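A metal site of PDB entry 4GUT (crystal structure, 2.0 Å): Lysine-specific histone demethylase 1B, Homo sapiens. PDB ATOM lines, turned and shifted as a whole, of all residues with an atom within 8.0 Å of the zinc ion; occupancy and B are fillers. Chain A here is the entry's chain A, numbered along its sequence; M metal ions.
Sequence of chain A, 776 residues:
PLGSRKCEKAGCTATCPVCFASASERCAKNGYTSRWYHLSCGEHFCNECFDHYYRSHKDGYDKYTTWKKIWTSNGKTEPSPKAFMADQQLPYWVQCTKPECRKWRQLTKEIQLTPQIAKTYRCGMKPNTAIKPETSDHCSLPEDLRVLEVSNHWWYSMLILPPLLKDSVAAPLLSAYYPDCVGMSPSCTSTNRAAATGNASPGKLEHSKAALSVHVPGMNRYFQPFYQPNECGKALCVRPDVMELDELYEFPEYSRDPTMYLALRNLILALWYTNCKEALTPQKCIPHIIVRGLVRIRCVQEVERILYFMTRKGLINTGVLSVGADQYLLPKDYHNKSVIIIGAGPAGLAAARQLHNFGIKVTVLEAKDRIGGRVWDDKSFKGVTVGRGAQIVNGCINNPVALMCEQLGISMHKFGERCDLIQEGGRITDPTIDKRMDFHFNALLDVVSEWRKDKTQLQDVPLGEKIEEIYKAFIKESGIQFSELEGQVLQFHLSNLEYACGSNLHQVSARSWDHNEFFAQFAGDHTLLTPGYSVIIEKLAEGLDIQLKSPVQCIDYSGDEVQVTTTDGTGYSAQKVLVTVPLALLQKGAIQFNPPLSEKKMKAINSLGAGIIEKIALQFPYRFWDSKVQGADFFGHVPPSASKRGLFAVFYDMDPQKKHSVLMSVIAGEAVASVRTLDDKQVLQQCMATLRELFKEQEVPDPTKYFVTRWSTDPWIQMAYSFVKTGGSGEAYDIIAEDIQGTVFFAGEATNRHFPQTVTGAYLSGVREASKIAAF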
ATOM      1  N   LYS A   6      -7.554  12.773   7.068  1.00  0.00           N
ATOM      2  CA  LYS A   6      -8.060  13.353   8.301  1.00  0.00           C
ATOM      3  C   LYS A   6      -9.544  13.086   8.455  1.00  0.00           C
ATOM      4  O   LYS A   6     -10.306  13.121   7.482  1.00  0.00           O
ATOM      5  CB  LYS A   6      -7.769  14.852   8.372  1.00  0.00           C
ATOM      6  CG  LYS A   6      -6.461  15.217   9.060  1.00  0.00           C
ATOM      7  CD  LYS A   6      -6.536  14.980  10.562  1.00  0.00           C
ATOM      8  CE  LYS A   6      -5.175  14.624  11.131  1.00  0.00           C
ATOM      9  NZ  LYS A   6      -5.265  14.071  12.510  1.00  0.00           N
ATOM     10  N   CYS A   7      -9.960  12.821   9.693  1.00  0.00           N
ATOM     11  CA  CYS A   7     -11.354  12.623  10.027  1.00  0.00           C
ATOM     12  C   CYS A   7     -12.147  13.928   9.914  1.00  0.00           C
ATOM     13  O   CYS A   7     -11.627  15.002  10.234  1.00  0.00           O
ATOM     14  CB  CYS A   7     -11.472  12.069  11.452  1.00  0.00           C
ATOM     15  SG  CYS A   7     -13.167  11.869  12.043  1.00  0.00           S
ATOM     16  N   GLU A   8     -13.392  13.818   9.466  1.00  0.00           N
ATOM     17  CA  GLU A   8     -14.331  14.943   9.431  1.00  0.00           C
ATOM     18  C   GLU A   8     -14.447  15.646  10.789  1.00  0.00           C
ATOM     19  O   GLU A   8     -14.482  16.885  10.852  1.00  0.00           O
ATOM     20  CB  GLU A   8     -15.716  14.470   8.966  1.00  0.00           C
ATOM     21  CG  GLU A   8     -16.495  13.696  10.034  1.00  0.00           C
ATOM     22  CD  GLU A   8     -17.792  13.085   9.532  1.00  0.00           C
ATOM     23  OE1 GLU A   8     -18.267  12.123  10.171  1.00  0.00           O
ATOM     24  OE2 GLU A   8     -18.346  13.555   8.519  1.00  0.00           O
ATOM     25  N   LYS A   9     -14.488  14.859  11.863  1.00  0.00           N
ATOM     26  CA  LYS A   9     -14.822  15.341  13.197  1.00  0.00           C
ATOM     27  C   LYS A   9     -13.700  16.152  13.832  1.00  0.00           C
ATOM     28  O   LYS A   9     -12.574  15.665  13.969  1.00  0.00           O
ATOM     29  CB  LYS A   9     -15.196  14.162  14.118  1.00  0.00           C
ATOM     30  CG  LYS A   9     -15.987  14.537  15.359  1.00  0.00           C
ATOM     31  CD  LYS A   9     -17.469  14.688  15.043  1.00  0.00           C
ATOM     32  CE  LYS A   9     -18.254  15.185  16.244  1.00  0.00           C
ATOM     33  NZ  LYS A   9     -19.708  15.317  15.931  1.00  0.00           N
ATOM     34  N   ALA A  10     -14.014  17.383  14.209  1.00  0.00           N
ATOM     35  CA  ALA A  10     -13.082  18.250  14.905  1.00  0.00           C
ATOM     36  C   ALA A  10     -12.741  17.668  16.276  1.00  0.00           C
ATOM     37  O   ALA A  10     -13.619  17.209  17.006  1.00  0.00           O
ATOM     38  CB  ALA A  10     -13.655  19.650  15.045  1.00  0.00           C
ATOM     39  N   GLY A  11     -11.451  17.654  16.587  1.00  0.00           N
ATOM     40  CA  GLY A  11     -10.957  17.171  17.875  1.00  0.00           C
ATOM     41  C   GLY A  11     -10.724  15.670  17.950  1.00  0.00           C
ATOM     42  O   GLY A  11     -10.276  15.168  18.985  1.00  0.00           O
ATOM     43  N   CYS A  12     -11.031  14.958  16.874  1.00  0.00           N
ATOM     44  CA  CYS A  12     -10.817  13.506  16.825  1.00  0.00           C
ATOM     45  C   CYS A  12      -9.343  13.137  16.867  1.00  0.00           C
ATOM     46  O   CYS A  12      -8.502  13.783  16.233  1.00  0.00           O
ATOM     47  CB  CYS A  12     -11.484  12.880  15.595  1.00  0.00           C
ATOM     48  SG  CYS A  12     -11.113  11.112  15.409  1.00  0.00           S
ATOM     49  N   THR A  13      -9.039  12.073  17.600  1.00  0.00           N
ATOM     50  CA  THR A  13      -7.664  11.695  17.905  1.00  0.00           C
ATOM     51  C   THR A  13      -7.078  10.637  16.950  1.00  0.00           C
ATOM     52  O   THR A  13      -5.918  10.234  17.096  1.00  0.00           O
ATOM     53  CB  THR A  13      -7.531  11.240  19.384  1.00  0.00           C
ATOM     54  OG1 THR A  13      -6.152  11.072  19.718  1.00  0.00           O
ATOM     55  CG2 THR A  13      -8.301   9.946  19.636  1.00  0.00           C
ATOM     56  N   ALA A  14      -7.881  10.218  15.979  1.00  0.00           N
ATOM     57  CA  ALA A  14      -7.451   9.206  14.998  1.00  0.00           C
ATOM     58  C   ALA A  14      -6.510   9.783  13.943  1.00  0.00           C
ATOM     59  O   ALA A  14      -6.949  10.447  12.990  1.00  0.00           O
ATOM     60  CB  ALA A  14      -8.643   8.535  14.355  1.00  0.00           C
ATOM     61  N   THR A  15      -5.212   9.537  14.126  1.00  0.00           N
ATOM     62  CA  THR A  15      -4.183   9.990  13.198  1.00  0.00           C
ATOM     63  C   THR A  15      -4.256   9.238  11.858  1.00  0.00           C
ATOM     64  O   THR A  15      -3.935   9.806  10.812  1.00  0.00           O
ATOM     65  CB  THR A  15      -2.769   9.836  13.794  1.00  0.00           C
ATOM     66  OG1 THR A  15      -2.549   8.475  14.175  1.00  0.00           O
ATOM     67  CG2 THR A  15      -2.597  10.731  15.017  1.00  0.00           C
ATOM     68  N   PRO A  17      -7.237   6.999   9.970  1.00  0.00           N
ATOM     69  CA  PRO A  17      -8.541   6.363   9.822  1.00  0.00           C
ATOM     70  C   PRO A  17      -8.545   5.253   8.766  1.00  0.00           C
ATOM     71  O   PRO A  17      -8.110   5.480   7.635  1.00  0.00           O
ATOM     72  CB  PRO A  17      -9.445   7.522   9.357  1.00  0.00           C
ATOM     73  CG  PRO A  17      -8.635   8.769   9.458  1.00  0.00           C
ATOM     74  CD  PRO A  17      -7.210   8.330   9.344  1.00  0.00           C
ATOM     75  N   TRP A  36     -13.797  11.063   5.577  1.00  0.00           N
ATOM     76  CA  TRP A  36     -13.777  10.031   6.603  1.00  0.00           C
ATOM     77  C   TRP A  36     -14.867  10.260   7.601  1.00  0.00           C
ATOM     78  O   TRP A  36     -14.865  11.268   8.316  1.00  0.00           O
ATOM     79  CB  TRP A  36     -12.422   9.986   7.290  1.00  0.00           C
ATOM     80  CG  TRP A  36     -11.391   9.178   6.545  1.00  0.00           C
ATOM     81  CD1 TRP A  36     -10.182   9.616   6.011  1.00  0.00           C
ATOM     82  CD2 TRP A  36     -11.472   7.743   6.205  1.00  0.00           C
ATOM     83  NE1 TRP A  36      -9.525   8.581   5.385  1.00  0.00           N
ATOM     84  CE2 TRP A  36     -10.239   7.439   5.465  1.00  0.00           C
ATOM     85  CE3 TRP A  36     -12.390   6.736   6.434  1.00  0.00           C
ATOM     86  CZ2 TRP A  36      -9.968   6.158   4.993  1.00  0.00           C
ATOM     87  CZ3 TRP A  36     -12.110   5.451   5.947  1.00  0.00           C
ATOM     88  CH2 TRP A  36     -10.932   5.170   5.243  1.00  0.00           C
ATOM     89  N   TYR A  37     -15.813   9.322   7.658  1.00  0.00           N
ATOM     90  CA  TYR A  37     -16.958   9.424   8.570  1.00  0.00           C
ATOM     91  C   TYR A  37     -16.640   8.885   9.956  1.00  0.00           C
ATOM     92  O   TYR A  37     -16.051   7.820  10.095  1.00  0.00           O
ATOM     93  CB  TYR A  37     -18.188   8.753   7.974  1.00  0.00           C
ATOM     94  CG  TYR A  37     -18.708   9.500   6.772  1.00  0.00           C
ATOM     95  CD1 TYR A  37     -19.583  10.583   6.928  1.00  0.00           C
ATOM     96  CD2 TYR A  37     -18.297   9.170   5.481  1.00  0.00           C
ATOM     97  CE1 TYR A  37     -20.063  11.288   5.832  1.00  0.00           C
ATOM     98  CE2 TYR A  37     -18.768   9.865   4.380  1.00  0.00           C
ATOM     99  CZ  TYR A  37     -19.647  10.918   4.564  1.00  0.00           C
ATOM    100  OH  TYR A  37     -20.126  11.626   3.482  1.00  0.00           O
ATOM    101  N   HIS A  38     -17.060   9.632  10.968  1.00  0.00           N
ATOM    102  CA  HIS A  38     -16.677   9.381  12.341  1.00  0.00           C
ATOM    103  C   HIS A  38     -17.814   8.800  13.145  1.00  0.00           C
ATOM    104  O   HIS A  38     -18.773   9.502  13.443  1.00  0.00           O
ATOM    105  CB  HIS A  38     -16.158  10.674  12.971  1.00  0.00           C
ATOM    106  CG  HIS A  38     -15.888  10.571  14.446  1.00  0.00           C
ATOM    107  ND1 HIS A  38     -14.655  10.400  14.937  1.00  0.00           N
ATOM    108  CD2 HIS A  38     -16.747  10.632  15.538  1.00  0.00           C
ATOM    109  CE1 HIS A  38     -14.716  10.361  16.282  1.00  0.00           C
ATOM    110  NE2 HIS A  38     -15.993  10.502  16.640  1.00  0.00           N
ATOM    111  N   LEU A  39     -17.696   7.516  13.475  1.00  0.00           N
ATOM    112  CA  LEU A  39     -18.592   6.869  14.439  1.00  0.00           C
ATOM    113  C   LEU A  39     -18.039   6.973  15.850  1.00  0.00           C
ATOM    114  O   LEU A  39     -18.783   7.233  16.791  1.00  0.00           O
ATOM    115  CB  LEU A  39     -18.823   5.395  14.054  1.00  0.00           C
ATOM    116  CG  LEU A  39     -20.237   4.983  13.616  1.00  0.00           C
ATOM    117  CD1 LEU A  39     -20.930   6.057  12.797  1.00  0.00           C
ATOM    118  CD2 LEU A  39     -20.198   3.674  12.851  1.00  0.00           C
ATOM    119  N   SER A  40     -16.724   6.787  15.990  1.00  0.00           N
ATOM    120  CA  SER A  40     -16.009   7.002  17.242  1.00  0.00           C
ATOM    121  C   SER A  40     -14.551   7.339  16.953  1.00  0.00           C
ATOM    122  O   SER A  40     -14.106   7.241  15.815  1.00  0.00           O
ATOM    123  CB  SER A  40     -16.082   5.755  18.123  1.00  0.00           C
ATOM    124  OG  SER A  40     -15.094   4.806  17.749  1.00  0.00           O
ATOM    125  N   CYS A  41     -13.815   7.697  18.001  1.00  0.00           N
ATOM    126  CA  CYS A  41     -12.380   7.964  17.880  1.00  0.00           C
ATOM    127  C   CYS A  41     -11.568   6.817  17.250  1.00  0.00           C
ATOM    128  O   CYS A  41     -10.453   7.032  16.768  1.00  0.00           O
ATOM    129  CB  CYS A  41     -11.787   8.336  19.240  1.00  0.00           C
ATOM    130  SG  CYS A  41     -12.071  10.060  19.689  1.00  0.00           S
ATOM    131  N   GLY A  42     -12.144   5.613  17.237  1.00  0.00           N
ATOM    132  CA  GLY A  42     -11.486   4.442  16.654  1.00  0.00           C
ATOM    133  C   GLY A  42     -12.223   3.796  15.491  1.00  0.00           C
ATOM    134  O   GLY A  42     -11.772   2.776  14.959  1.00  0.00           O
ATOM    135  N   GLU A  43     -13.338   4.377  15.081  1.00  0.00           N
ATOM    136  CA  GLU A  43     -14.163   3.783  14.030  1.00  0.00           C
ATOM    137  C   GLU A  43     -14.632   4.793  13.003  1.00  0.00           C
ATOM    138  O   GLU A  43     -15.349   5.736  13.326  1.00  0.00           O
ATOM    139  CB  GLU A  43     -15.363   3.053  14.638  1.00  0.00           C
ATOM    140  CG  GLU A  43     -15.003   1.772  15.353  1.00  0.00           C
ATOM    141  CD  GLU A  43     -15.906   1.457  16.533  1.00  0.00           C
ATOM    142  OE1 GLU A  43     -16.091   0.260  16.819  1.00  0.00           O
ATOM    143  OE2 GLU A  43     -16.413   2.409  17.184  1.00  0.00           O
ATOM    144  N   HIS A  44     -14.222   4.568  11.756  1.00  0.00           N
ATOM    145  CA  HIS A  44     -14.641   5.412  10.634  1.00  0.00           C
ATOM    146  C   HIS A  44     -14.932   4.589   9.428  1.00  0.00           C
ATOM    147  O   HIS A  44     -14.426   3.480   9.271  1.00  0.00           O
ATOM    148  CB  HIS A  44     -13.548   6.412  10.292  1.00  0.00           C
ATOM    149  CG  HIS A  44     -13.023   7.186  11.468  1.00  0.00           C
ATOM    150  ND1 HIS A  44     -12.085   6.701  12.300  1.00  0.00           N
ATOM    151  CD2 HIS A  44     -13.347   8.453  11.939  1.00  0.00           C
ATOM    152  CE1 HIS A  44     -11.823   7.612  13.252  1.00  0.00           C
ATOM    153  NE2 HIS A  44     -12.598   8.680  13.034  1.00  0.00           N
ATOM    154  N   MET A 158     -16.994  11.783  22.230  1.00  0.00           N
ATOM    155  CA  MET A 158     -16.606  11.736  20.811  1.00  0.00           C
ATOM    156  C   MET A 158     -17.269  10.601  20.039  1.00  0.00           C
ATOM    157  O   MET A 158     -17.087  10.467  18.828  1.00  0.00           O
ATOM    158  CB  MET A 158     -15.075  11.651  20.682  1.00  0.00           C
ATOM    159  CG  MET A 158     -14.360  12.986  20.824  1.00  0.00           C
ATOM    160  SD  MET A 158     -14.303  13.958  19.298  1.00  0.00           S
ATOM    161  CE  MET A 158     -15.935  14.685  19.218  1.00  0.00           C
HETATM  162 ZN    ZN M   1     -12.628  10.556  14.024  1.00  0.00          ZN
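N of His 38 sits at hydrogen-bond distance from OE1 of Glu 8, at 2.9 Å.
The backbone NH of Ala 14 lies close to the side-chain sulfur of Cys 12 (3.4 Å).
O of Met 158 is in hydrogen-bond range of NE2 of His 38.
A ring nitrogen (NE2) of His 44 lies close to the backbone carbonyl oxygen (O) of Ser 40 (3.5 Å).
O of Ser 40 sits close to ND1 of His 38 (3.3 Å).
The side-chain sulfur of Cys 7 sits close to the backbone NH of Lys 9 (3.3 Å).
The nearest printed residue that does not touch the zinc ion is Ser 40 (4.05 Å).
The zinc ion is bound by NE2 of His 44 (2.1 Å), SG of Cys 12 (2.1 Å), ND1 of His 38 (2.2 Å) and SG of Cys 7 (2.4 Å).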
